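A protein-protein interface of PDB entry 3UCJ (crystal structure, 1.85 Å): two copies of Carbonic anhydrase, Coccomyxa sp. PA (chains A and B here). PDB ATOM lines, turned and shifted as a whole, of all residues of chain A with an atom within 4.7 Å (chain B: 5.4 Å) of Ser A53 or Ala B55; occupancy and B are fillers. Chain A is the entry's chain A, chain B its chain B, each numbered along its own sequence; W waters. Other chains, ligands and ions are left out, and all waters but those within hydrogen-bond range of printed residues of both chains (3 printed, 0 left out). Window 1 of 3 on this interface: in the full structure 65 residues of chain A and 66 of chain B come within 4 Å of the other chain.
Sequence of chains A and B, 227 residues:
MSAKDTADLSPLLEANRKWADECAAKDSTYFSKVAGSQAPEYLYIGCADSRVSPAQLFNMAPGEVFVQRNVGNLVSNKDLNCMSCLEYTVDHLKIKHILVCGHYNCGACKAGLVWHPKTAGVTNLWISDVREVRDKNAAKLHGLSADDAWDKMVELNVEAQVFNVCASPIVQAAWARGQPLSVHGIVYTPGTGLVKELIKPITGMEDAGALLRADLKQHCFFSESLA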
ATOM      1  N   ARG A  51     -29.925  -6.529  23.335  1.00  0.00           N
ATOM      2  CA  ARG A  51     -30.752  -5.330  23.351  1.00  0.00           C
ATOM      3  C   ARG A  51     -29.964  -4.089  23.682  1.00  0.00           C
ATOM      4  O   ARG A  51     -30.549  -2.968  23.793  1.00  0.00           O
ATOM      5  CB  ARG A  51     -31.889  -5.528  24.329  1.00  0.00           C
ATOM      6  CG  ARG A  51     -32.793  -6.573  23.838  1.00  0.00           C
ATOM      7  CD  ARG A  51     -33.749  -7.010  24.970  1.00  0.00           C
ATOM      8  NE  ARG A  51     -33.055  -7.603  26.142  1.00  0.00           N
ATOM      9  CZ  ARG A  51     -33.638  -7.833  27.323  1.00  0.00           C
ATOM     10  NH1 ARG A  51     -34.942  -7.473  27.545  1.00  0.00           N
ATOM     11  NH2 ARG A  51     -32.903  -8.325  28.332  1.00  0.00           N
ATOM     12  N   VAL A  52     -28.651  -4.264  23.888  1.00  0.00           N
ATOM     13  CA  VAL A  52     -27.868  -3.193  24.510  1.00  0.00           C
ATOM     14  C   VAL A  52     -26.587  -2.873  23.689  1.00  0.00           C
ATOM     15  O   VAL A  52     -25.478  -3.400  24.002  1.00  0.00           O
ATOM     16  CB  VAL A  52     -27.438  -3.549  25.969  1.00  0.00           C
ATOM     17  CG1 VAL A  52     -26.902  -2.303  26.717  1.00  0.00           C
ATOM     18  CG2 VAL A  52     -28.635  -4.246  26.749  1.00  0.00           C
ATOM     19  N   SER A  53     -26.729  -1.963  22.709  1.00  0.00           N
ATOM     20  CA  SER A  53     -25.594  -1.642  21.815  1.00  0.00           C
ATOM     21  C   SER A  53     -24.997  -0.246  22.126  1.00  0.00           C
ATOM     22  O   SER A  53     -25.669   0.774  21.881  1.00  0.00           O
ATOM     23  CB  SER A  53     -26.083  -1.703  20.382  1.00  0.00           C
ATOM     24  OG  SER A  53     -25.080  -1.177  19.545  1.00  0.00           O
ATOM     25  N   PRO A  54     -23.762  -0.189  22.655  1.00  0.00           N
ATOM     26  CA  PRO A  54     -23.310   1.064  23.225  1.00  0.00           C
ATOM     27  C   PRO A  54     -23.193   2.180  22.150  1.00  0.00           C
ATOM     28  O   PRO A  54     -23.597   3.349  22.412  1.00  0.00           O
ATOM     29  CB  PRO A  54     -21.927   0.722  23.804  1.00  0.00           C
ATOM     30  CG  PRO A  54     -21.606  -0.612  23.339  1.00  0.00           C
ATOM     31  CD  PRO A  54     -22.897  -1.313  23.067  1.00  0.00           C
ATOM     32  N   ALA A  55     -22.688   1.846  20.955  1.00  0.00           N
ATOM     33  CA  ALA A  55     -22.529   2.951  19.974  1.00  0.00           C
ATOM     34  C   ALA A  55     -23.880   3.492  19.476  1.00  0.00           C
ATOM     35  O   ALA A  55     -24.065   4.709  19.403  1.00  0.00           O
ATOM     36  CB  ALA A  55     -21.570   2.587  18.805  1.00  0.00           C
ATOM     37  N   GLN A  56     -24.811   2.610  19.164  1.00  0.00           N
ATOM     38  CA  GLN A  56     -26.210   3.006  18.891  1.00  0.00           C
ATOM     39  C   GLN A  56     -26.787   3.833  20.033  1.00  0.00           C
ATOM     40  O   GLN A  56     -27.173   5.011  19.824  1.00  0.00           O
ATOM     41  CB  GLN A  56     -27.132   1.795  18.639  1.00  0.00           C
ATOM     42  CG  GLN A  56     -26.622   0.909  17.521  1.00  0.00           C
ATOM     43  CD  GLN A  56     -27.744   0.209  16.790  1.00  0.00           C
ATOM     44  OE1 GLN A  56     -28.672  -0.387  17.413  1.00  0.00           O
ATOM     45  NE2 GLN A  56     -27.704   0.296  15.452  1.00  0.00           N
ATOM     46  N   LEU A  57     -26.795   3.295  21.258  1.00  0.00           N
ATOM     47  CA  LEU A  57     -27.552   4.002  22.305  1.00  0.00           C
ATOM     48  C   LEU A  57     -26.965   5.345  22.702  1.00  0.00           C
ATOM     49  O   LEU A  57     -27.685   6.223  23.231  1.00  0.00           O
ATOM     50  CB  LEU A  57     -27.808   3.126  23.535  1.00  0.00           C
ATOM     51  CG  LEU A  57     -26.620   2.825  24.437  1.00  0.00           C
ATOM     52  CD1 LEU A  57     -26.649   3.788  25.543  1.00  0.00           C
ATOM     53  CD2 LEU A  57     -26.757   1.354  24.953  1.00  0.00           C
ATOM     54  N   ARG A  69     -17.826  -6.577  25.927  1.00  0.00           N
ATOM     55  CA  ARG A  69     -19.198  -6.942  26.317  1.00  0.00           C
ATOM     56  C   ARG A  69     -19.135  -8.431  26.654  1.00  0.00           C
ATOM     57  O   ARG A  69     -18.535  -9.194  25.929  1.00  0.00           O
ATOM     58  CB  ARG A  69     -20.165  -6.741  25.125  1.00  0.00           C
ATOM     59  CG  ARG A  69     -20.599  -5.234  25.049  1.00  0.00           C
ATOM     60  CD  ARG A  69     -21.439  -5.083  23.780  1.00  0.00           C
ATOM     61  NE  ARG A  69     -22.762  -5.768  23.862  1.00  0.00           N
ATOM     62  CZ  ARG A  69     -23.708  -5.649  22.949  1.00  0.00           C
ATOM     63  NH1 ARG A  69     -23.532  -4.910  21.824  1.00  0.00           N
ATOM     64  NH2 ARG A  69     -24.806  -6.318  23.112  1.00  0.00           N
ATOM     65  N   SER B  53     -18.581  -1.516  15.317  1.00  0.00           N
ATOM     66  CA  SER B  53     -19.728  -1.715  16.182  1.00  0.00           C
ATOM     67  C   SER B  53     -20.756  -2.555  15.420  1.00  0.00           C
ATOM     68  O   SER B  53     -21.399  -2.027  14.512  1.00  0.00           O
ATOM     69  CB  SER B  53     -20.263  -0.311  16.533  1.00  0.00           C
ATOM     70  OG  SER B  53     -21.586  -0.499  17.045  1.00  0.00           O
ATOM     71  N   PRO B  54     -20.945  -3.868  15.763  1.00  0.00           N
ATOM     72  CA  PRO B  54     -21.738  -4.758  14.963  1.00  0.00           C
ATOM     73  C   PRO B  54     -23.183  -4.313  14.703  1.00  0.00           C
ATOM     74  O   PRO B  54     -23.628  -4.438  13.553  1.00  0.00           O
ATOM     75  CB  PRO B  54     -21.759  -6.074  15.772  1.00  0.00           C
ATOM     76  CG  PRO B  54     -21.403  -5.654  17.148  1.00  0.00           C
ATOM     77  CD  PRO B  54     -20.430  -4.545  16.966  1.00  0.00           C
ATOM     78  N   ALA B  55     -23.907  -3.847  15.702  1.00  0.00           N
ATOM     79  CA  ALA B  55     -25.362  -3.574  15.468  1.00  0.00           C
ATOM     80  C   ALA B  55     -25.524  -2.361  14.517  1.00  0.00           C
ATOM     81  O   ALA B  55     -26.480  -2.283  13.660  1.00  0.00           O
ATOM     82  CB  ALA B  55     -26.100  -3.326  16.767  1.00  0.00           C
ATOM     83  N   GLN B  56     -24.637  -1.406  14.728  1.00  0.00           N
ATOM     84  CA  GLN B  56     -24.563  -0.194  13.886  1.00  0.00           C
ATOM     85  C   GLN B  56     -24.198  -0.528  12.452  1.00  0.00           C
ATOM     86  O   GLN B  56     -24.919  -0.151  11.498  1.00  0.00           O
ATOM     87  CB  GLN B  56     -23.553   0.757  14.530  1.00  0.00           C
ATOM     88  CG  GLN B  56     -23.617   2.164  14.038  1.00  0.00           C
ATOM     89  CD  GLN B  56     -22.494   3.002  14.628  1.00  0.00           C
ATOM     90  OE1 GLN B  56     -21.294   2.781  14.371  1.00  0.00           O
ATOM     91  NE2 GLN B  56     -22.887   3.963  15.455  1.00  0.00           N
ATOM     92  N   LEU B  57     -23.138  -1.328  12.267  1.00  0.00           N
ATOM     93  CA  LEU B  57     -22.650  -1.610  10.933  1.00  0.00           C
ATOM     94  C   LEU B  57     -23.550  -2.542  10.160  1.00  0.00           C
ATOM     95  O   LEU B  57     -23.509  -2.588   8.948  1.00  0.00           O
ATOM     96  CB  LEU B  57     -21.179  -2.045  10.992  1.00  0.00           C
ATOM     97  CG  LEU B  57     -20.867  -3.494  11.494  1.00  0.00           C
ATOM     98  CD1 LEU B  57     -20.938  -4.342  10.333  1.00  0.00           C
ATOM     99  CD2 LEU B  57     -19.422  -3.439  12.018  1.00  0.00           C
ATOM    100  N   PHE B  58     -24.396  -3.295  10.848  1.00  0.00           N
ATOM    101  CA  PHE B  58     -25.408  -4.131  10.170  1.00  0.00           C
ATOM    102  C   PHE B  58     -26.782  -3.466  10.178  1.00  0.00           C
ATOM    103  O   PHE B  58     -27.744  -4.048   9.692  1.00  0.00           O
ATOM    104  CB  PHE B  58     -25.500  -5.547  10.779  1.00  0.00           C
ATOM    105  CG  PHE B  58     -24.333  -6.414  10.426  1.00  0.00           C
ATOM    106  CD1 PHE B  58     -24.055  -6.669   9.113  1.00  0.00           C
ATOM    107  CD2 PHE B  58     -23.489  -6.993  11.457  1.00  0.00           C
ATOM    108  CE1 PHE B  58     -22.953  -7.426   8.753  1.00  0.00           C
ATOM    109  CE2 PHE B  58     -22.422  -7.778  11.121  1.00  0.00           C
ATOM    110  CZ  PHE B  58     -22.137  -8.001   9.760  1.00  0.00           C
ATOM    111  N   ASN B  59     -26.856  -2.256  10.701  1.00  0.00           N
ATOM    112  CA  ASN B  59     -28.121  -1.498  10.799  1.00  0.00           C
ATOM    113  C   ASN B  59     -29.242  -2.291  11.500  1.00  0.00           C
ATOM    114  O   ASN B  59     -30.416  -2.351  11.049  1.00  0.00           O
ATOM    115  CB  ASN B  59     -28.561  -1.003   9.420  1.00  0.00           C
ATOM    116  CG  ASN B  59     -29.558   0.173   9.523  1.00  0.00           C
ATOM    117  OD1 ASN B  59     -30.620   0.123   8.935  1.00  0.00           O
ATOM    118  ND2 ASN B  59     -29.248   1.154  10.342  1.00  0.00           N
ATOM    119  N   MET B  60     -28.862  -2.941  12.605  1.00  0.00           N
ATOM    120  CA  MET B  60     -29.797  -3.724  13.389  1.00  0.00           C
ATOM    121  C   MET B  60     -30.441  -2.921  14.499  1.00  0.00           C
ATOM    122  O   MET B  60     -29.834  -2.038  15.090  1.00  0.00           O
ATOM    123  CB  MET B  60     -29.106  -4.992  13.930  1.00  0.00           C
ATOM    124  CG  MET B  60     -28.862  -5.978  12.840  1.00  0.00           C
ATOM    125  SD  MET B  60     -27.675  -7.117  13.580  1.00  0.00           S
ATOM    126  CE  MET B  60     -27.857  -8.530  12.587  1.00  0.00           C
ATOM    127  N   VAL B  65     -28.777  -8.898  17.633  1.00  0.00           N
ATOM    128  CA  VAL B  65     -27.421  -9.504  17.644  1.00  0.00           C
ATOM    129  C   VAL B  65     -26.868  -9.456  19.089  1.00  0.00           C
ATOM    130  O   VAL B  65     -26.755  -8.438  19.716  1.00  0.00           O
ATOM    131  CB  VAL B  65     -26.427  -8.888  16.601  1.00  0.00           C
ATOM    132  CG1 VAL B  65     -26.253  -7.357  16.837  1.00  0.00           C
ATOM    133  CG2 VAL B  65     -25.034  -9.600  16.602  1.00  0.00           C
HETATM  134  O   HOH W   1     -21.578  -0.636  19.869  1.00  0.00           O
HETATM  135  O   HOH W   2     -23.452  -3.427  18.582  1.00  0.00           O
HETATM  136  O   HOH W   3     -25.918  -5.698  20.193  1.00  0.00           O
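Water W1 lies within hydrogen-bond range of the side-chain hydroxyl (OG) of Ser B53 (2.8 Å) and the backbone NH (N) of Ala A55 (2.9 Å). Water W3 lies within hydrogen-bond range of the backbone carbonyl oxygen of Val B65 (2.9 Å) and the guanidinium group of Arg A69 (3.0 Å). Water W2 lies within hydrogen-bond range of OG of Ser A53 and N of Ala B55.
Ser A53 touches Ala B55. CB of Ala A55 touches OG of Ser B53, 3.6 Å away. Ala A55 touches Gln B56. Gln A56 touches Gln B56 (NE2 to CA, 3.5 Å).
Of chain B, only Ala B55 (3.7 Å) comes within 4 Å of Ser A53. Printed residues of chain B within 4 Å of Ala A55: Ser B53 and Gln B56. Printed residues of chain B within 4 Å of Gln A56: Ala B55, Gln B56 and Met B60. Of the printed residues of chain A, Ser B53 touches Ala A55. Ala B55 touches just these residues of chain A: Ser A53 (3.7 Å) and Gln A56 (3.4 Å). Of the printed residues of chain A, Gln B56 touches Ala A55 (3.9 Å) and Gln A56 (3.5 Å). Printed residues of chain A within 4 Å of Met B60: Gln A56 (3.1 Å). The nearest residue of chain B that does not touch Ser A53 is Ser B53 (4.3 Å). The nearest printed residue of chain A that does not touch Ala B55 is Arg A69 (5.9 Å). The nearest printed residue of chain A that does not touch Met B60 is Ser A53 (6.5 Å).
Ser A53 touches Ala B55, and with the chains exchanged Ala A55 touches Ser B53. Ala A55 touches Gln B56, and with the chains exchanged Gln A56 touches Ala B55. Gln A56 touches its own counterpart, Gln B56. Positions printed for both chains: 53, 54, 55, 56 and 57. Of the 6 pairs that touch across the chains among the printed residues, 5 have their exchanged pair printed and touching as well.
The side-chain amide nitrogen (NE2) of Gln A56 lies within hydrogen-bond range of the backbone carbonyl oxygen (O) of Ala B55. The side-chain amide oxygen (OE1) of Gln A56 lies close to the backbone carbonyl oxygen (O) of Met B60, 3.1 Å away.
Of the 9 printed residues of chain B, 4 touch a printed residue of chain A. Hydrophobic or aromatic side chains of chain B within 4 Å of the printed part of chain A: Ala B55. Of the 8 printed residues of chain A, 3 touch a printed residue of chain B. Hydrophobic or aromatic side chains of chain A within 4 Å of the printed part of chain B: Ala A55. Among the printed residues, no Asp or Glu carboxylate lies within 4 Å of a Lys or Arg side-chain nitrogen of the other chain.
The backbone carbonyl oxygen (O) of Ala B55 sits at hydrogen-bond distance from the backbone NH (N) of Met B60, 2.7 Å away.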
